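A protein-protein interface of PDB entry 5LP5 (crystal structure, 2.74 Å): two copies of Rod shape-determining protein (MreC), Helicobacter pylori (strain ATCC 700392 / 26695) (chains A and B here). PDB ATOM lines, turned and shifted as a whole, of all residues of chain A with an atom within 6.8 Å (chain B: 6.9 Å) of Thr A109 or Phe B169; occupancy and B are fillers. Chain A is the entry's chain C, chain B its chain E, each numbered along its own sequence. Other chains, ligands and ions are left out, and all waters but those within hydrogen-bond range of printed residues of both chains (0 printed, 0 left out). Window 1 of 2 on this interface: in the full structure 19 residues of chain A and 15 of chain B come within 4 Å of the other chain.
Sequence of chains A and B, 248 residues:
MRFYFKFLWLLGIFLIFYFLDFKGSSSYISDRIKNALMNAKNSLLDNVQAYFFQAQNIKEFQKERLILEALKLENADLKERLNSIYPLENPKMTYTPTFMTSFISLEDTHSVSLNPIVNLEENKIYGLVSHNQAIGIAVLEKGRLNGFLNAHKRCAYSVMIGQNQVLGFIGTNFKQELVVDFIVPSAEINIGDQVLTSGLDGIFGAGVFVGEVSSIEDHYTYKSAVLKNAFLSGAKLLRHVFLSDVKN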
ATOM      1  N   MET A 100      20.934  -9.698 -15.478  1.00  0.00           N
ATOM      2  CA  MET A 100      20.121 -10.902 -15.451  1.00  0.00           C
ATOM      3  C   MET A 100      20.936 -12.069 -14.916  1.00  0.00           C
ATOM      4  O   MET A 100      22.101 -12.219 -15.221  1.00  0.00           O
ATOM      5  CB  MET A 100      19.484 -11.193 -16.817  1.00  0.00           C
ATOM      6  CG  MET A 100      20.381 -11.828 -17.850  1.00  0.00           C
ATOM      7  SD  MET A 100      19.530 -12.007 -19.427  1.00  0.00           S
ATOM      8  CE  MET A 100      18.700 -13.582 -19.192  1.00  0.00           C
ATOM      9  N   PHE A 103      17.202 -16.736 -17.468  1.00  0.00           N
ATOM     10  CA  PHE A 103      15.845 -16.576 -17.998  1.00  0.00           C
ATOM     11  C   PHE A 103      14.887 -17.175 -16.970  1.00  0.00           C
ATOM     12  O   PHE A 103      15.290 -18.029 -16.181  1.00  0.00           O
ATOM     13  CB  PHE A 103      15.707 -17.304 -19.311  1.00  0.00           C
ATOM     14  CG  PHE A 103      16.513 -16.708 -20.411  1.00  0.00           C
ATOM     15  CD1 PHE A 103      15.978 -15.754 -21.258  1.00  0.00           C
ATOM     16  CD2 PHE A 103      17.810 -17.145 -20.641  1.00  0.00           C
ATOM     17  CE1 PHE A 103      16.741 -15.244 -22.292  1.00  0.00           C
ATOM     18  CE2 PHE A 103      18.576 -16.628 -21.667  1.00  0.00           C
ATOM     19  CZ  PHE A 103      18.042 -15.676 -22.493  1.00  0.00           C
ATOM     20  N   SER A 105      11.892 -18.856 -17.708  1.00  0.00           N
ATOM     21  CA  SER A 105      11.596 -20.161 -18.283  1.00  0.00           C
ATOM     22  C   SER A 105      12.723 -20.432 -19.255  1.00  0.00           C
ATOM     23  O   SER A 105      13.370 -19.481 -19.696  1.00  0.00           O
ATOM     24  CB  SER A 105      10.270 -20.096 -19.036  1.00  0.00           C
ATOM     25  OG  SER A 105       9.842 -21.388 -19.393  1.00  0.00           O
ATOM     26  N   LEU A 106      12.970 -21.696 -19.599  1.00  0.00           N
ATOM     27  CA  LEU A 106      13.863 -22.014 -20.708  1.00  0.00           C
ATOM     28  C   LEU A 106      13.116 -22.228 -21.996  1.00  0.00           C
ATOM     29  O   LEU A 106      13.701 -22.631 -22.981  1.00  0.00           O
ATOM     30  CB  LEU A 106      14.746 -23.232 -20.411  1.00  0.00           C
ATOM     31  CG  LEU A 106      15.839 -22.956 -19.366  1.00  0.00           C
ATOM     32  CD1 LEU A 106      16.625 -24.215 -19.081  1.00  0.00           C
ATOM     33  CD2 LEU A 106      16.834 -21.890 -19.797  1.00  0.00           C
ATOM     34  N   GLU A 107      11.819 -21.966 -21.962  1.00  0.00           N
ATOM     35  CA  GLU A 107      10.977 -22.000 -23.137  1.00  0.00           C
ATOM     36  C   GLU A 107      10.478 -20.605 -23.514  1.00  0.00           C
ATOM     37  O   GLU A 107       9.462 -20.478 -24.208  1.00  0.00           O
ATOM     38  CB  GLU A 107       9.753 -22.900 -22.872  1.00  0.00           C
ATOM     39  CG  GLU A 107      10.051 -24.394 -22.718  1.00  0.00           C
ATOM     40  CD  GLU A 107       8.874 -25.185 -22.196  1.00  0.00           C
ATOM     41  OE1 GLU A 107       7.716 -24.901 -22.586  1.00  0.00           O
ATOM     42  OE2 GLU A 107       9.108 -26.124 -21.401  1.00  0.00           O
ATOM     43  N   ASP A 108      11.157 -19.550 -23.063  1.00  0.00           N
ATOM     44  CA  ASP A 108      10.715 -18.168 -23.303  1.00  0.00           C
ATOM     45  C   ASP A 108      11.919 -17.229 -23.146  1.00  0.00           C
ATOM     46  O   ASP A 108      12.485 -17.145 -22.036  1.00  0.00           O
ATOM     47  CB  ASP A 108       9.594 -17.839 -22.306  1.00  0.00           C
ATOM     48  CG  ASP A 108       9.002 -16.434 -22.465  1.00  0.00           C
ATOM     49  OD1 ASP A 108       9.055 -15.853 -23.566  1.00  0.00           O
ATOM     50  OD2 ASP A 108       8.516 -15.910 -21.434  1.00  0.00           O
ATOM     51  N   THR A 109      12.291 -16.548 -24.239  1.00  0.00           N
ATOM     52  CA  THR A 109      13.437 -15.629 -24.241  1.00  0.00           C
ATOM     53  C   THR A 109      13.087 -14.208 -23.789  1.00  0.00           C
ATOM     54  O   THR A 109      13.960 -13.375 -23.621  1.00  0.00           O
ATOM     55  CB  THR A 109      14.031 -15.469 -25.668  1.00  0.00           C
ATOM     56  OG1 THR A 109      13.057 -14.900 -26.561  1.00  0.00           O
ATOM     57  CG2 THR A 109      14.517 -16.795 -26.226  1.00  0.00           C
ATOM     58  N   HIS A 110      11.787 -13.940 -23.644  1.00  0.00           N
ATOM     59  CA  HIS A 110      11.309 -12.605 -23.329  1.00  0.00           C
ATOM     60  C   HIS A 110      11.005 -12.422 -21.832  1.00  0.00           C
ATOM     61  O   HIS A 110      10.296 -11.473 -21.474  1.00  0.00           O
ATOM     62  CB  HIS A 110      10.065 -12.285 -24.178  1.00  0.00           C
ATOM     63  CG  HIS A 110      10.200 -12.650 -25.628  1.00  0.00           C
ATOM     64  ND1 HIS A 110      10.912 -11.902 -26.537  1.00  0.00           N
ATOM     65  CD2 HIS A 110       9.731 -13.719 -26.308  1.00  0.00           C
ATOM     66  CE1 HIS A 110      10.862 -12.489 -27.720  1.00  0.00           C
ATOM     67  NE2 HIS A 110      10.140 -13.588 -27.610  1.00  0.00           N
ATOM     68  N   SER A 111      11.566 -13.249 -20.961  1.00  0.00           N
ATOM     69  CA  SER A 111      11.314 -13.135 -19.530  1.00  0.00           C
ATOM     70  C   SER A 111      12.568 -13.501 -18.764  1.00  0.00           C
ATOM     71  O   SER A 111      13.110 -14.606 -18.937  1.00  0.00           O
ATOM     72  CB  SER A 111      10.168 -14.052 -19.098  1.00  0.00           C
ATOM     73  OG  SER A 111       8.920 -13.513 -19.495  1.00  0.00           O
ATOM     74  N   VAL A 112      13.042 -12.595 -17.907  1.00  0.00           N
ATOM     75  CA  VAL A 112      14.292 -12.833 -17.195  1.00  0.00           C
ATOM     76  C   VAL A 112      14.240 -12.518 -15.707  1.00  0.00           C
ATOM     77  O   VAL A 112      13.496 -11.637 -15.267  1.00  0.00           O
ATOM     78  CB  VAL A 112      15.452 -12.033 -17.824  1.00  0.00           C
ATOM     79  CG1 VAL A 112      15.624 -12.404 -19.281  1.00  0.00           C
ATOM     80  CG2 VAL A 112      15.235 -10.533 -17.670  1.00  0.00           C
ATOM     81  N   LEU A 149      10.530  -8.505 -21.214  1.00  0.00           N
ATOM     82  CA  LEU A 149      11.183  -7.832 -22.327  1.00  0.00           C
ATOM     83  C   LEU A 149      10.212  -7.505 -23.455  1.00  0.00           C
ATOM     84  O   LEU A 149       9.059  -7.909 -23.435  1.00  0.00           O
ATOM     85  CB  LEU A 149      12.325  -8.699 -22.852  1.00  0.00           C
ATOM     86  CG  LEU A 149      13.358  -9.115 -21.792  1.00  0.00           C
ATOM     87  CD1 LEU A 149      14.427 -10.005 -22.396  1.00  0.00           C
ATOM     88  CD2 LEU A 149      14.007  -7.913 -21.118  1.00  0.00           C
ATOM     89  N   GLN A 176       5.250 -12.213 -32.667  1.00  0.00           N
ATOM     90  CA  GLN A 176       6.188 -11.572 -31.743  1.00  0.00           C
ATOM     91  C   GLN A 176       7.006 -10.423 -32.368  1.00  0.00           C
ATOM     92  O   GLN A 176       8.230 -10.335 -32.187  1.00  0.00           O
ATOM     93  CB  GLN A 176       7.100 -12.622 -31.090  1.00  0.00           C
ATOM     94  CG  GLN A 176       6.364 -13.492 -30.087  1.00  0.00           C
ATOM     95  CD  GLN A 176       7.180 -14.662 -29.607  1.00  0.00           C
ATOM     96  OE1 GLN A 176       7.782 -15.405 -30.405  1.00  0.00           O
ATOM     97  NE2 GLN A 176       7.195 -14.844 -28.290  1.00  0.00           N
ATOM     98  N   PHE A 231      14.705  -3.738 -30.208  1.00  0.00           N
ATOM     99  CA  PHE A 231      15.256  -4.883 -29.515  1.00  0.00           C
ATOM    100  C   PHE A 231      14.249  -6.012 -29.465  1.00  0.00           C
ATOM    101  O   PHE A 231      13.126  -5.821 -29.010  1.00  0.00           O
ATOM    102  CB  PHE A 231      15.655  -4.535 -28.074  1.00  0.00           C
ATOM    103  CG  PHE A 231      16.019  -5.743 -27.267  1.00  0.00           C
ATOM    104  CD1 PHE A 231      17.246  -6.356 -27.442  1.00  0.00           C
ATOM    105  CD2 PHE A 231      15.110  -6.312 -26.384  1.00  0.00           C
ATOM    106  CE1 PHE A 231      17.570  -7.503 -26.742  1.00  0.00           C
ATOM    107  CE2 PHE A 231      15.415  -7.453 -25.697  1.00  0.00           C
ATOM    108  CZ  PHE A 231      16.657  -8.035 -25.846  1.00  0.00           C
ATOM    109  N   LEU A 232      14.653  -7.186 -29.937  1.00  0.00           N
ATOM    110  CA  LEU A 232      13.907  -8.438 -29.680  1.00  0.00           C
ATOM    111  C   LEU A 232      14.781  -9.545 -29.071  1.00  0.00           C
ATOM    112  O   LEU A 232      14.746  -9.769 -27.880  1.00  0.00           O
ATOM    113  CB  LEU A 232      13.202  -8.983 -30.963  1.00  0.00           C
ATOM    114  CG  LEU A 232      11.984  -8.213 -31.472  1.00  0.00           C
ATOM    115  CD1 LEU A 232      11.475  -8.775 -32.781  1.00  0.00           C
ATOM    116  CD2 LEU A 232      10.875  -8.228 -30.425  1.00  0.00           C
ATOM    117  N   SER A 233      15.529 -10.247 -29.924  1.00  0.00           N
ATOM    118  CA  SER A 233      16.100 -11.542 -29.634  1.00  0.00           C
ATOM    119  C   SER A 233      17.599 -11.357 -29.493  1.00  0.00           C
ATOM    120  O   SER A 233      18.296 -12.341 -29.553  1.00  0.00           O
ATOM    121  CB  SER A 233      15.805 -12.477 -30.869  1.00  0.00           C
ATOM    122  OG  SER A 233      15.423 -13.849 -30.626  1.00  0.00           O
ATOM    123  N   LEU A 238      21.339  -7.709 -23.594  1.00  0.00           N
ATOM    124  CA  LEU A 238      20.881  -8.247 -22.327  1.00  0.00           C
ATOM    125  C   LEU A 238      21.968  -8.102 -21.273  1.00  0.00           C
ATOM    126  O   LEU A 238      21.738  -8.319 -20.085  1.00  0.00           O
ATOM    127  CB  LEU A 238      20.338  -9.664 -22.497  1.00  0.00           C
ATOM    128  CG  LEU A 238      18.887  -9.696 -23.020  1.00  0.00           C
ATOM    129  CD1 LEU A 238      18.385 -11.113 -23.270  1.00  0.00           C
ATOM    130  CD2 LEU A 238      17.909  -8.989 -22.085  1.00  0.00           C
ATOM    131  N   ALA B 156      18.595 -28.637 -21.878  1.00  0.00           N
ATOM    132  CA  ALA B 156      18.273 -27.374 -22.527  1.00  0.00           C
ATOM    133  C   ALA B 156      19.160 -26.252 -21.991  1.00  0.00           C
ATOM    134  O   ALA B 156      19.508 -26.232 -20.812  1.00  0.00           O
ATOM    135  CB  ALA B 156      16.812 -27.036 -22.306  1.00  0.00           C
ATOM    136  N   TYR B 157      19.515 -25.308 -22.842  1.00  0.00           N
ATOM    137  CA  TYR B 157      20.297 -24.149 -22.387  1.00  0.00           C
ATOM    138  C   TYR B 157      20.297 -23.066 -23.452  1.00  0.00           C
ATOM    139  O   TYR B 157      19.909 -23.340 -24.617  1.00  0.00           O
ATOM    140  CB  TYR B 157      21.729 -24.555 -22.048  1.00  0.00           C
ATOM    141  CG  TYR B 157      22.458 -25.352 -23.123  1.00  0.00           C
ATOM    142  CD1 TYR B 157      23.227 -24.717 -24.095  1.00  0.00           C
ATOM    143  CD2 TYR B 157      22.403 -26.721 -23.153  1.00  0.00           C
ATOM    144  CE1 TYR B 157      23.922 -25.426 -25.053  1.00  0.00           C
ATOM    145  CE2 TYR B 157      23.083 -27.447 -24.117  1.00  0.00           C
ATOM    146  CZ  TYR B 157      23.859 -26.796 -25.060  1.00  0.00           C
ATOM    147  OH  TYR B 157      24.531 -27.524 -26.023  1.00  0.00           O
ATOM    148  N   SER B 158      20.766 -21.870 -23.068  1.00  0.00           N
ATOM    149  CA  SER B 158      20.690 -20.690 -23.936  1.00  0.00           C
ATOM    150  C   SER B 158      21.876 -20.510 -24.857  1.00  0.00           C
ATOM    151  O   SER B 158      23.024 -20.506 -24.416  1.00  0.00           O
ATOM    152  CB  SER B 158      20.540 -19.416 -23.126  1.00  0.00           C
ATOM    153  OG  SER B 158      20.305 -18.309 -23.974  1.00  0.00           O
ATOM    154  N   VAL B 159      21.578 -20.333 -26.140  1.00  0.00           N
ATOM    155  CA  VAL B 159      22.600 -20.160 -27.153  1.00  0.00           C
ATOM    156  C   VAL B 159      22.294 -18.911 -27.979  1.00  0.00           C
ATOM    157  O   VAL B 159      21.169 -18.370 -27.971  1.00  0.00           O
ATOM    158  CB  VAL B 159      22.700 -21.375 -28.078  1.00  0.00           C
ATOM    159  CG1 VAL B 159      23.095 -22.597 -27.290  1.00  0.00           C
ATOM    160  CG2 VAL B 159      21.393 -21.629 -28.831  1.00  0.00           C
ATOM    161  N   LEU B 167      19.050 -15.022 -30.130  1.00  0.00           N
ATOM    162  CA  LEU B 167      18.817 -15.954 -29.031  1.00  0.00           C
ATOM    163  C   LEU B 167      17.831 -17.061 -29.348  1.00  0.00           C
ATOM    164  O   LEU B 167      16.844 -16.867 -30.076  1.00  0.00           O
ATOM    165  CB  LEU B 167      18.309 -15.186 -27.805  1.00  0.00           C
ATOM    166  CG  LEU B 167      19.355 -14.309 -27.122  1.00  0.00           C
ATOM    167  CD1 LEU B 167      18.695 -13.428 -26.075  1.00  0.00           C
ATOM    168  CD2 LEU B 167      20.445 -15.170 -26.496  1.00  0.00           C
ATOM    169  N   GLY B 168      18.111 -18.218 -28.769  1.00  0.00           N
ATOM    170  CA  GLY B 168      17.217 -19.364 -28.837  1.00  0.00           C
ATOM    171  C   GLY B 168      17.566 -20.276 -27.669  1.00  0.00           C
ATOM    172  O   GLY B 168      18.397 -19.916 -26.797  1.00  0.00           O
ATOM    173  N   PHE B 169      16.937 -21.444 -27.627  1.00  0.00           N
ATOM    174  CA  PHE B 169      17.265 -22.444 -26.620  1.00  0.00           C
ATOM    175  C   PHE B 169      17.496 -23.792 -27.278  1.00  0.00           C
ATOM    176  O   PHE B 169      16.823 -24.174 -28.232  1.00  0.00           O
ATOM    177  CB  PHE B 169      16.149 -22.595 -25.588  1.00  0.00           C
ATOM    178  CG  PHE B 169      15.942 -21.389 -24.730  1.00  0.00           C
ATOM    179  CD1 PHE B 169      16.754 -21.155 -23.640  1.00  0.00           C
ATOM    180  CD2 PHE B 169      14.899 -20.525 -24.977  1.00  0.00           C
ATOM    181  CE1 PHE B 169      16.562 -20.060 -22.827  1.00  0.00           C
ATOM    182  CE2 PHE B 169      14.687 -19.434 -24.157  1.00  0.00           C
ATOM    183  CZ  PHE B 169      15.526 -19.199 -23.082  1.00  0.00           C
ATOM    184  N   ILE B 170      18.424 -24.544 -26.717  1.00  0.00           N
ATOM    185  CA  ILE B 170      18.744 -25.851 -27.253  1.00  0.00           C
ATOM    186  C   ILE B 170      17.641 -26.837 -26.904  1.00  0.00           C
ATOM    187  O   ILE B 170      17.205 -26.897 -25.765  1.00  0.00           O
ATOM    188  CB  ILE B 170      20.114 -26.348 -26.744  1.00  0.00           C
ATOM    189  CG1 ILE B 170      21.249 -25.641 -27.517  1.00  0.00           C
ATOM    190  CG2 ILE B 170      20.233 -27.860 -26.904  1.00  0.00           C
ATOM    191  CD1 ILE B 170      21.444 -26.096 -28.948  1.00  0.00           C
ATOM    192  N   GLY B 171      17.168 -27.560 -27.897  1.00  0.00           N
ATOM    193  CA  GLY B 171      16.240 -28.639 -27.671  1.00  0.00           C
ATOM    194  C   GLY B 171      16.485 -29.713 -28.699  1.00  0.00           C
ATOM    195  O   GLY B 171      17.599 -29.929 -29.141  1.00  0.00           O
ATOM    196  N   THR B 172      15.412 -30.378 -29.087  1.00  0.00           N
ATOM    197  CA  THR B 172      15.471 -31.473 -30.048  1.00  0.00           C
ATOM    198  C   THR B 172      14.104 -31.585 -30.712  1.00  0.00           C
ATOM    199  O   THR B 172      13.195 -30.825 -30.369  1.00  0.00           O
ATOM    200  CB  THR B 172      15.904 -32.781 -29.361  1.00  0.00           C
ATOM    201  OG1 THR B 172      16.078 -33.804 -30.325  1.00  0.00           O
ATOM    202  CG2 THR B 172      14.901 -33.241 -28.342  1.00  0.00           C
ATOM    203  N   VAL B 179      18.542 -29.150 -32.058  1.00  0.00           N
ATOM    204  CA  VAL B 179      17.861 -28.010 -32.624  1.00  0.00           C
ATOM    205  C   VAL B 179      18.046 -26.782 -31.738  1.00  0.00           C
ATOM    206  O   VAL B 179      18.106 -26.898 -30.502  1.00  0.00           O
ATOM    207  CB  VAL B 179      16.375 -28.350 -32.742  1.00  0.00           C
ATOM    208  CG1 VAL B 179      15.542 -27.144 -33.052  1.00  0.00           C
ATOM    209  CG2 VAL B 179      16.166 -29.312 -33.870  1.00  0.00           C
ATOM    210  N   VAL B 180      18.115 -25.603 -32.362  1.00  0.00           N
ATOM    211  CA  VAL B 180      17.882 -24.354 -31.635  1.00  0.00           C
ATOM    212  C   VAL B 180      16.434 -23.942 -31.857  1.00  0.00           C
ATOM    213  O   VAL B 180      15.979 -23.757 -32.980  1.00  0.00           O
ATOM    214  CB  VAL B 180      18.807 -23.212 -32.051  1.00  0.00           C
ATOM    215  CG1 VAL B 180      18.466 -21.931 -31.281  1.00  0.00           C
ATOM    216  CG2 VAL B 180      20.254 -23.604 -31.816  1.00  0.00           C
ATOM    217  N   ASP B 181      15.718 -23.810 -30.749  1.00  0.00           N
ATOM    218  CA  ASP B 181      14.289 -23.608 -30.746  1.00  0.00           C
ATOM    219  C   ASP B 181      13.993 -22.214 -30.216  1.00  0.00           C
ATOM    220  O   ASP B 181      14.880 -21.545 -29.662  1.00  0.00           O
ATOM    221  CB  ASP B 181      13.695 -24.639 -29.791  1.00  0.00           C
ATOM    222  CG  ASP B 181      12.267 -24.919 -30.036  1.00  0.00           C
ATOM    223  OD1 ASP B 181      11.551 -24.080 -30.636  1.00  0.00           O
ATOM    224  OD2 ASP B 181      11.871 -26.014 -29.593  1.00  0.00           O
ATOM    225  N   PHE B 182      12.744 -21.774 -30.364  1.00  0.00           N
ATOM    226  CA  PHE B 182      12.252 -20.534 -29.744  1.00  0.00           C
ATOM    227  C   PHE B 182      12.826 -19.243 -30.345  1.00  0.00           C
ATOM    228  O   PHE B 182      12.970 -18.251 -29.634  1.00  0.00           O
ATOM    229  CB  PHE B 182      12.505 -20.581 -28.227  1.00  0.00           C
ATOM    230  CG  PHE B 182      11.794 -21.719 -27.549  1.00  0.00           C
ATOM    231  CD1 PHE B 182      10.410 -21.750 -27.545  1.00  0.00           C
ATOM    232  CD2 PHE B 182      12.480 -22.729 -26.877  1.00  0.00           C
ATOM    233  CE1 PHE B 182       9.729 -22.774 -26.920  1.00  0.00           C
ATOM    234  CE2 PHE B 182      11.811 -23.767 -26.274  1.00  0.00           C
ATOM    235  CZ  PHE B 182      10.437 -23.783 -26.279  1.00  0.00           C
ATOM    236  N   ILE B 183      13.110 -19.243 -31.651  1.00  0.00           N
ATOM    237  CA  ILE B 183      13.657 -18.070 -32.304  1.00  0.00           C
ATOM    238  C   ILE B 183      12.537 -17.231 -32.892  1.00  0.00           C
ATOM    239  O   ILE B 183      11.614 -17.748 -33.498  1.00  0.00           O
ATOM    240  CB  ILE B 183      14.614 -18.430 -33.445  1.00  0.00           C
ATOM    241  CG1 ILE B 183      15.619 -19.499 -33.013  1.00  0.00           C
ATOM    242  CG2 ILE B 183      15.374 -17.181 -33.856  1.00  0.00           C
ATOM    243  CD1 ILE B 183      16.283 -20.205 -34.180  1.00  0.00           C
ATOM    244  N   VAL B 184      12.631 -15.914 -32.720  1.00  0.00           N
ATOM    245  CA  VAL B 184      11.647 -15.008 -33.290  1.00  0.00           C
ATOM    246  C   VAL B 184      11.666 -15.126 -34.815  1.00  0.00           C
ATOM    247  O   VAL B 184      12.726 -15.195 -35.429  1.00  0.00           O
ATOM    248  CB  VAL B 184      11.877 -13.546 -32.860  1.00  0.00           C
ATOM    249  CG1 VAL B 184      11.685 -13.404 -31.359  1.00  0.00           C
ATOM    250  CG2 VAL B 184      13.251 -13.051 -33.270  1.00  0.00           C
ATOM    251  N   ASP B 201      22.276 -17.638 -19.203  1.00  0.00           N
ATOM    252  CA  ASP B 201      21.378 -18.572 -18.502  1.00  0.00           C
ATOM    253  C   ASP B 201      21.858 -19.031 -17.122  1.00  0.00           C
ATOM    254  O   ASP B 201      21.121 -19.682 -16.385  1.00  0.00           O
ATOM    255  CB  ASP B 201      21.077 -19.798 -19.367  1.00  0.00           C
ATOM    256  CG  ASP B 201      22.323 -20.488 -19.898  1.00  0.00           C
ATOM    257  OD1 ASP B 201      23.448 -20.056 -19.595  1.00  0.00           O
ATOM    258  OD2 ASP B 201      22.166 -21.476 -20.643  1.00  0.00           O
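Of the printed residues of chain B, Leu A106 touches Ala B156 (3.9 Å), Phe B169 (3.1 Å) and Phe B182 (3.96 Å). Of the printed residues of chain B, Glu A107 touches Phe B182 (3.6 Å). Of the printed residues of chain B, Asp A108 touches Phe B169. Of the printed residues of chain B, Thr A109 touches Phe B169 (3.4 Å). Of the printed residues of chain A, Ser B158 touches Phe A103. Of the printed residues of chain A, Phe B169 touches Phe A103, Leu A106, Asp A108 and Thr A109. Of the printed residues of chain A, Phe B182 touches Leu A106 (3.96 Å) and Glu A107 (3.6 Å). The nearest printed residue of chain A that does not touch Val B184 is Gln A176 (4.5 Å).
Among the printed residues, merely in contact across the chains: Phe A103 with Ser B158 (3.3 Å), Phe A103 with Phe B169 (3.8 Å), Leu A106 with Ala B156 (3.9 Å), Leu A106 with Phe B169 (3.1 Å), Leu A106 with Phe B182 (3.96 Å), Glu A107 with Phe B182 (3.6 Å), Asp A108 with Phe B169 (3.7 Å), Thr A109 with Phe B169 (3.4 Å), His A110 with Val B184 (3.8 Å), Ser A233 with Val B184 (3.5 Å) and Leu A238 with Leu B167 (3.7 Å).
The side-chain hydroxyl (OG) of Ser A105 lies close to the backbone NH (N) of Glu A107 (3.3 Å). N of His A110 lies close to OD1 of Asp A108 (3.3 Å). OD2 of Asp A108 lies within hydrogen-bond range of OG of Ser A111, at 3.1 Å. The side-chain hydroxyl (OG1) of Thr A109 lies within hydrogen-bond range of a ring nitrogen (NE2) of His A110 (3.4 Å). The backbone NH of Leu A149 sits at hydrogen-bond distance from the backbone carbonyl oxygen of His A110, 3.0 Å away. The backbone NH (N) of Ser B158 sits at hydrogen-bond distance from the side-chain carboxylate (OD2) of Asp B201.
No position is printed for both chains. Of the 12 pairs that touch across the chains among the printed residues, none has its exchanged pair printed and touching as well.
Hydrophobic or aromatic side chains of chain B within 4 Å of the printed part of chain A: Leu B167, Phe B169, Phe B182 and Val B184. Of the 16 printed residues of chain A, 8 touch a printed residue of chain B. Hydrophobic or aromatic side chains of chain A that line the printed part of chain B: Phe A103, Leu A106, His A110 and Leu A238. Among the printed residues, no Asp or Glu carboxylate lies within 4 Å of a Lys or Arg side-chain nitrogen of the other chain.
The backbone carbonyl oxygen (O) of Ser A233 is in hydrogen-bond range of the backbone NH (N) of Leu B167 (2.8 Å).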
